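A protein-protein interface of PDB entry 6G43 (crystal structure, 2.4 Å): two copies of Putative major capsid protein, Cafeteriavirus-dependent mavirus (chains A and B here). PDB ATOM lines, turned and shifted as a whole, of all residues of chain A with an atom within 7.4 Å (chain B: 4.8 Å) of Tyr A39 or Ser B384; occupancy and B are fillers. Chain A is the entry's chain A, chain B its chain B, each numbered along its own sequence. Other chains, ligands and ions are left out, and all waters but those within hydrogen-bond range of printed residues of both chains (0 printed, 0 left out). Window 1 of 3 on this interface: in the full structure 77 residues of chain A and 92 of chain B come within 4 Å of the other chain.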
ATOM      1  N   ARG A  34      -3.873 -11.805  36.041  1.00  0.00           N
ATOM      2  CA  ARG A  34      -2.868 -11.960  34.994  1.00  0.00           C
ATOM      3  C   ARG A  34      -1.429 -11.742  35.459  1.00  0.00           C
ATOM      4  O   ARG A  34      -1.151 -10.917  36.335  1.00  0.00           O
ATOM      5  CB  ARG A  34      -3.184 -11.000  33.842  1.00  0.00           C
ATOM      6  CG  ARG A  34      -2.456 -11.310  32.541  1.00  0.00           C
ATOM      7  CD  ARG A  34      -2.796 -10.296  31.465  1.00  0.00           C
ATOM      8  NE  ARG A  34      -4.156 -10.469  30.946  1.00  0.00           N
ATOM      9  CZ  ARG A  34      -4.498 -11.148  29.845  1.00  0.00           C
ATOM     10  NH1 ARG A  34      -3.590 -11.757  29.080  1.00  0.00           N
ATOM     11  NH2 ARG A  34      -5.782 -11.216  29.498  1.00  0.00           N
ATOM     12  N   GLY A  36       2.301 -11.472  32.938  1.00  0.00           N
ATOM     13  CA  GLY A  36       2.711 -11.330  31.542  1.00  0.00           C
ATOM     14  C   GLY A  36       4.158 -10.913  31.411  1.00  0.00           C
ATOM     15  O   GLY A  36       4.808 -10.577  32.400  1.00  0.00           O
ATOM     16  N   ILE A  37       4.656 -10.953  30.178  1.00  0.00           N
ATOM     17  CA  ILE A  37       6.004 -10.498  29.859  1.00  0.00           C
ATOM     18  C   ILE A  37       6.002  -8.967  29.927  1.00  0.00           C
ATOM     19  O   ILE A  37       5.365  -8.329  29.090  1.00  0.00           O
ATOM     20  CB  ILE A  37       6.448 -10.995  28.463  1.00  0.00           C
ATOM     21  CG1 ILE A  37       6.515 -12.529  28.455  1.00  0.00           C
ATOM     22  CG2 ILE A  37       7.805 -10.403  28.074  1.00  0.00           C
ATOM     23  CD1 ILE A  37       6.635 -13.145  27.079  1.00  0.00           C
ATOM     24  N   PRO A  38       6.704  -8.373  30.920  1.00  0.00           N
ATOM     25  CA  PRO A  38       6.592  -6.918  31.096  1.00  0.00           C
ATOM     26  C   PRO A  38       7.299  -6.084  30.019  1.00  0.00           C
ATOM     27  O   PRO A  38       8.156  -6.595  29.291  1.00  0.00           O
ATOM     28  CB  PRO A  38       7.229  -6.665  32.476  1.00  0.00           C
ATOM     29  CG  PRO A  38       7.706  -7.982  32.985  1.00  0.00           C
ATOM     30  CD  PRO A  38       7.689  -8.954  31.850  1.00  0.00           C
ATOM     31  N   TYR A  39       6.913  -4.810  29.942  1.00  0.00           N
ATOM     32  CA  TYR A  39       7.491  -3.832  29.015  1.00  0.00           C
ATOM     33  C   TYR A  39       8.457  -2.853  29.705  1.00  0.00           C
ATOM     34  O   TYR A  39       8.941  -1.913  29.075  1.00  0.00           O
ATOM     35  CB  TYR A  39       6.366  -3.066  28.304  1.00  0.00           C
ATOM     36  CG  TYR A  39       5.759  -3.827  27.145  1.00  0.00           C
ATOM     37  CD1 TYR A  39       4.931  -4.929  27.365  1.00  0.00           C
ATOM     38  CD2 TYR A  39       6.014  -3.448  25.824  1.00  0.00           C
ATOM     39  CE1 TYR A  39       4.373  -5.631  26.305  1.00  0.00           C
ATOM     40  CE2 TYR A  39       5.460  -4.145  24.758  1.00  0.00           C
ATOM     41  CZ  TYR A  39       4.641  -5.234  25.002  1.00  0.00           C
ATOM     42  OH  TYR A  39       4.091  -5.927  23.950  1.00  0.00           O
ATOM     43  N   SER A  40       8.759  -3.090  30.983  1.00  0.00           N
ATOM     44  CA  SER A  40       9.744  -2.300  31.726  1.00  0.00           C
ATOM     45  C   SER A  40      11.167  -2.863  31.596  1.00  0.00           C
ATOM     46  O   SER A  40      12.075  -2.431  32.303  1.00  0.00           O
ATOM     47  CB  SER A  40       9.344  -2.267  33.202  1.00  0.00           C
ATOM     48  OG  SER A  40       9.283  -3.580  33.739  1.00  0.00           O
ATOM     49  N   THR A  41      11.354  -3.789  30.659  1.00  0.00           N
ATOM     50  CA  THR A  41      12.478  -4.714  30.650  1.00  0.00           C
ATOM     51  C   THR A  41      13.383  -4.605  29.410  1.00  0.00           C
ATOM     52  O   THR A  41      14.324  -5.390  29.264  1.00  0.00           O
ATOM     53  CB  THR A  41      11.923  -6.149  30.741  1.00  0.00           C
ATOM     54  OG1 THR A  41      10.940  -6.351  29.715  1.00  0.00           O
ATOM     55  CG2 THR A  41      11.281  -6.385  32.115  1.00  0.00           C
ATOM     56  N   PHE A  42      13.113  -3.637  28.532  1.00  0.00           N
ATOM     57  CA  PHE A  42      13.883  -3.471  27.305  1.00  0.00           C
ATOM     58  C   PHE A  42      15.241  -2.840  27.602  1.00  0.00           C
ATOM     59  O   PHE A  42      15.342  -1.954  28.451  1.00  0.00           O
ATOM     60  CB  PHE A  42      13.115  -2.608  26.297  1.00  0.00           C
ATOM     61  CG  PHE A  42      11.974  -3.324  25.630  1.00  0.00           C
ATOM     62  CD1 PHE A  42      10.706  -3.329  26.202  1.00  0.00           C
ATOM     63  CD2 PHE A  42      12.165  -3.996  24.424  1.00  0.00           C
ATOM     64  CE1 PHE A  42       9.652  -3.990  25.587  1.00  0.00           C
ATOM     65  CE2 PHE A  42      11.114  -4.658  23.802  1.00  0.00           C
ATOM     66  CZ  PHE A  42       9.855  -4.658  24.385  1.00  0.00           C
ATOM     67  N   LYS A 217       4.220 -13.652  17.365  1.00  0.00           N
ATOM     68  CA  LYS A 217       3.035 -13.344  18.169  1.00  0.00           C
ATOM     69  C   LYS A 217       3.308 -13.528  19.661  1.00  0.00           C
ATOM     70  O   LYS A 217       3.072 -12.617  20.459  1.00  0.00           O
ATOM     71  CB  LYS A 217       1.869 -14.246  17.760  1.00  0.00           C
ATOM     72  CG  LYS A 217       1.246 -13.892  16.419  1.00  0.00           C
ATOM     73  CD  LYS A 217      -0.008 -14.712  16.160  1.00  0.00           C
ATOM     74  CE  LYS A 217      -0.775 -14.196  14.951  1.00  0.00           C
ATOM     75  NZ  LYS A 217      -1.973 -15.031  14.657  1.00  0.00           N
ATOM     76  N   GLN A 271      14.524  -7.768  25.238  1.00  0.00           N
ATOM     77  CA  GLN A 271      13.815  -7.775  26.521  1.00  0.00           C
ATOM     78  C   GLN A 271      14.560  -8.708  27.462  1.00  0.00           C
ATOM     79  O   GLN A 271      14.896  -9.822  27.067  1.00  0.00           O
ATOM     80  CB  GLN A 271      12.393  -8.302  26.352  1.00  0.00           C
ATOM     81  CG  GLN A 271      11.466  -7.399  25.568  1.00  0.00           C
ATOM     82  CD  GLN A 271      10.076  -7.992  25.435  1.00  0.00           C
ATOM     83  OE1 GLN A 271       9.869  -8.935  24.671  1.00  0.00           O
ATOM     84  NE2 GLN A 271       9.115  -7.446  26.176  1.00  0.00           N
ATOM     85  N   PHE B 370       8.610   2.419  32.250  1.00  0.00           N
ATOM     86  CA  PHE B 370       8.506   2.691  30.804  1.00  0.00           C
ATOM     87  C   PHE B 370       9.312   3.895  30.282  1.00  0.00           C
ATOM     88  O   PHE B 370       9.101   4.310  29.138  1.00  0.00           O
ATOM     89  CB  PHE B 370       7.034   2.833  30.333  1.00  0.00           C
ATOM     90  CG  PHE B 370       6.149   1.648  30.628  1.00  0.00           C
ATOM     91  CD1 PHE B 370       6.650   0.351  30.742  1.00  0.00           C
ATOM     92  CD2 PHE B 370       4.772   1.835  30.726  1.00  0.00           C
ATOM     93  CE1 PHE B 370       5.800  -0.716  30.991  1.00  0.00           C
ATOM     94  CE2 PHE B 370       3.920   0.770  30.975  1.00  0.00           C
ATOM     95  CZ  PHE B 370       4.435  -0.509  31.105  1.00  0.00           C
ATOM     96  N   GLU B 372      12.409   4.080  29.348  1.00  0.00           N
ATOM     97  CA  GLU B 372      13.220   3.616  28.217  1.00  0.00           C
ATOM     98  C   GLU B 372      12.455   3.430  26.888  1.00  0.00           C
ATOM     99  O   GLU B 372      13.078   3.402  25.828  1.00  0.00           O
ATOM    100  CB  GLU B 372      13.990   2.329  28.593  1.00  0.00           C
ATOM    101  CG  GLU B 372      13.245   0.990  28.468  1.00  0.00           C
ATOM    102  CD  GLU B 372      12.118   0.782  29.478  1.00  0.00           C
ATOM    103  OE1 GLU B 372      11.936   1.627  30.385  1.00  0.00           O
ATOM    104  OE2 GLU B 372      11.410  -0.247  29.367  1.00  0.00           O
ATOM    105  N   LEU B 373      11.127   3.297  26.951  1.00  0.00           N
ATOM    106  CA  LEU B 373      10.309   2.994  25.771  1.00  0.00           C
ATOM    107  C   LEU B 373      10.163   4.166  24.793  1.00  0.00           C
ATOM    108  O   LEU B 373       9.831   5.281  25.192  1.00  0.00           O
ATOM    109  CB  LEU B 373       8.914   2.517  26.198  1.00  0.00           C
ATOM    110  CG  LEU B 373       8.821   1.238  27.042  1.00  0.00           C
ATOM    111  CD1 LEU B 373       7.367   0.810  27.176  1.00  0.00           C
ATOM    112  CD2 LEU B 373       9.649   0.107  26.449  1.00  0.00           C
ATOM    113  N   GLN B 377       7.709   0.766  20.626  1.00  0.00           N
ATOM    114  CA  GLN B 377       7.432  -0.128  21.754  1.00  0.00           C
ATOM    115  C   GLN B 377       6.146   0.250  22.491  1.00  0.00           C
ATOM    116  O   GLN B 377       5.444  -0.628  22.997  1.00  0.00           O
ATOM    117  CB  GLN B 377       8.623  -0.177  22.718  1.00  0.00           C
ATOM    118  CG  GLN B 377       9.748  -1.107  22.268  1.00  0.00           C
ATOM    119  CD  GLN B 377      10.354  -0.724  20.922  1.00  0.00           C
ATOM    120  OE1 GLN B 377      10.832   0.396  20.751  1.00  0.00           O
ATOM    121  NE2 GLN B 377      10.341  -1.654  19.961  1.00  0.00           N
ATOM    122  N   GLU B 380       3.556  -1.139  20.175  1.00  0.00           N
ATOM    123  CA  GLU B 380       3.553  -2.580  20.440  1.00  0.00           C
ATOM    124  C   GLU B 380       2.822  -2.928  21.741  1.00  0.00           C
ATOM    125  O   GLU B 380       2.051  -3.888  21.777  1.00  0.00           O
ATOM    126  CB  GLU B 380       4.990  -3.100  20.502  1.00  0.00           C
ATOM    127  CG  GLU B 380       5.122  -4.623  20.528  1.00  0.00           C
ATOM    128  CD  GLU B 380       6.536  -5.106  20.823  1.00  0.00           C
ATOM    129  OE1 GLU B 380       7.390  -4.296  21.245  1.00  0.00           O
ATOM    130  OE2 GLU B 380       6.793  -6.316  20.636  1.00  0.00           O
ATOM    131  N   LEU B 381       3.082  -2.148  22.792  1.00  0.00           N
ATOM    132  CA  LEU B 381       2.424  -2.299  24.097  1.00  0.00           C
ATOM    133  C   LEU B 381       0.913  -2.141  23.988  1.00  0.00           C
ATOM    134  O   LEU B 381       0.154  -2.998  24.445  1.00  0.00           O
ATOM    135  CB  LEU B 381       2.977  -1.262  25.086  1.00  0.00           C
ATOM    136  CG  LEU B 381       2.279  -1.058  26.440  1.00  0.00           C
ATOM    137  CD1 LEU B 381       2.161  -2.368  27.204  1.00  0.00           C
ATOM    138  CD2 LEU B 381       3.026  -0.025  27.274  1.00  0.00           C
ATOM    139  N   SER B 382       0.491  -1.029  23.390  1.00  0.00           N
ATOM    140  CA  SER B 382      -0.926  -0.728  23.214  1.00  0.00           C
ATOM    141  C   SER B 382      -1.631  -1.752  22.324  1.00  0.00           C
ATOM    142  O   SER B 382      -2.753  -2.162  22.624  1.00  0.00           O
ATOM    143  CB  SER B 382      -1.103   0.679  22.645  1.00  0.00           C
ATOM    144  OG  SER B 382      -2.435   1.120  22.810  1.00  0.00           O
ATOM    145  N   SER B 383      -0.967  -2.160  21.245  1.00  0.00           N
ATOM    146  CA  SER B 383      -1.497  -3.173  20.320  1.00  0.00           C
ATOM    147  C   SER B 383      -1.675  -4.548  20.967  1.00  0.00           C
ATOM    148  O   SER B 383      -2.649  -5.242  20.672  1.00  0.00           O
ATOM    149  CB  SER B 383      -0.605  -3.287  19.078  1.00  0.00           C
ATOM    150  OG  SER B 383      -0.679  -2.108  18.289  1.00  0.00           O
ATOM    151  N   SER B 384      -0.753  -4.927  21.853  1.00  0.00           N
ATOM    152  CA  SER B 384      -0.851  -6.190  22.593  1.00  0.00           C
ATOM    153  C   SER B 384      -2.022  -6.224  23.585  1.00  0.00           C
ATOM    154  O   SER B 384      -2.473  -7.303  23.965  1.00  0.00           O
ATOM    155  CB  SER B 384       0.466  -6.496  23.320  1.00  0.00           C
ATOM    156  OG  SER B 384       0.719  -5.572  24.367  1.00  0.00           O
ATOM    157  N   ASN B 385      -2.495  -5.047  24.005  1.00  0.00           N
ATOM    158  CA  ASN B 385      -3.689  -4.913  24.848  1.00  0.00           C
ATOM    159  C   ASN B 385      -4.956  -4.464  24.085  1.00  0.00           C
ATOM    160  O   ASN B 385      -5.898  -3.950  24.695  1.00  0.00           O
ATOM    161  CB  ASN B 385      -3.379  -3.948  25.998  1.00  0.00           C
ATOM    162  CG  ASN B 385      -2.273  -4.464  26.909  1.00  0.00           C
ATOM    163  OD1 ASN B 385      -2.329  -5.597  27.375  1.00  0.00           O
ATOM    164  ND2 ASN B 385      -1.269  -3.638  27.167  1.00  0.00           N
ATOM    165  N   GLY B 386      -4.979  -4.659  22.764  1.00  0.00           N
ATOM    166  CA  GLY B 386      -6.191  -4.472  21.957  1.00  0.00           C
ATOM    167  C   GLY B 386      -6.282  -3.256  21.045  1.00  0.00           C
ATOM    168  O   GLY B 386      -7.271  -3.119  20.321  1.00  0.00           O
ATOM    169  N   ASP B 432       2.118  -5.491  32.677  1.00  0.00           N
ATOM    170  CA  ASP B 432       3.081  -4.843  31.775  1.00  0.00           C
ATOM    171  C   ASP B 432       4.123  -3.988  32.513  1.00  0.00           C
ATOM    172  O   ASP B 432       5.236  -3.808  32.015  1.00  0.00           O
ATOM    173  CB  ASP B 432       2.367  -3.956  30.744  1.00  0.00           C
ATOM    174  CG  ASP B 432       1.458  -4.740  29.803  1.00  0.00           C
ATOM    175  OD1 ASP B 432       1.842  -5.832  29.335  1.00  0.00           O
ATOM    176  OD2 ASP B 432       0.355  -4.239  29.509  1.00  0.00           O
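OG of Ser B384 sits at hydrogen-bond distance from OH of Tyr A39 (3.4 Å). The backbone carbonyl oxygen of Asp B432 is in hydrogen-bond range of the backbone NH of Tyr A39 (2.8 Å). The side-chain carboxylate (OE2) of Glu B372 lies close to the backbone carbonyl oxygen (O) of Tyr A39.
The backbone carbonyl oxygen of Pro A38 is in hydrogen-bond range of the side-chain hydroxyl of Thr A41, 2.8 Å away. NE2 of Gln A271 sits at hydrogen-bond distance from O of Pro A38, at 3.4 Å. The backbone carbonyl oxygen of Glu B380 lies within hydrogen-bond range of the side-chain hydroxyl of Ser B384 (3.4 Å). The backbone carbonyl oxygen (O) of Leu B381 is in hydrogen-bond range of the side-chain hydroxyl (OG) of Ser B384 (2.6 Å). The side-chain amide nitrogen (ND2) of Asn B385 lies within hydrogen-bond range of the backbone carbonyl oxygen (O) of Leu B381 (3.1 Å). OD2 of Asp B432 is in hydrogen-bond range of ND2 of Asn B385 (2.9 Å).
Tyr A39 touches Phe B370 (CB to CE1, 3.6 Å). CD2 of Leu B373 touches O of Tyr A39 (3.4 Å). CE2 of Tyr A39 touches O of Gln B377, at 3.9 Å. Tyr A39 touches Glu B380. Tyr A39 touches Leu B381. Ser A40 touches Phe B370 (N to CE1, 3.8 Å). Ser A40 touches Glu B372. O of Asp B432 touches N of Ser A40 (3.7 Å). Thr A41 touches Glu B372 (N to OE2, 3.8 Å). CD1 of Phe A42 touches CD2 of Leu B373, 3.6 Å away.
Of chain B, only Phe B370 (3.6 Å), Glu B372 (3.0 Å), Leu B373 (3.4 Å), Gln B377 (3.9 Å), Glu B380 (3.6 Å), Leu B381 (3.6 Å), Ser B384 (3.4 Å) and Asp B432 (2.8 Å) come within 4 Å of Tyr A39. Printed residues of chain B within 4 Å of Ser A40: Phe B370, Glu B372 and Asp B432. Of the printed residues of chain B, Phe A42 touches Glu B372 and Leu B373. Of the printed residues of chain A, Phe B370 touches Tyr A39 (3.6 Å) and Ser A40 (3.8 Å). Ser B383 touches none of the printed residues of chain A. Printed residues of chain A within 4 Å of Ser B384: Tyr A39. Asn B385 touches none of the printed residues of chain A.
Printed residues of chain A that touch a printed residue of chain B: Pro A38, Tyr A39, Ser A40, Thr A41 and Phe A42. Hydrophobic or aromatic side chains of chain A within 4 Å of the printed part of chain B: Pro A38, Tyr A39 and Phe A42. Of the 12 printed residues of chain B, 8 touch a printed residue of chain A.
No position is printed for both chains.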
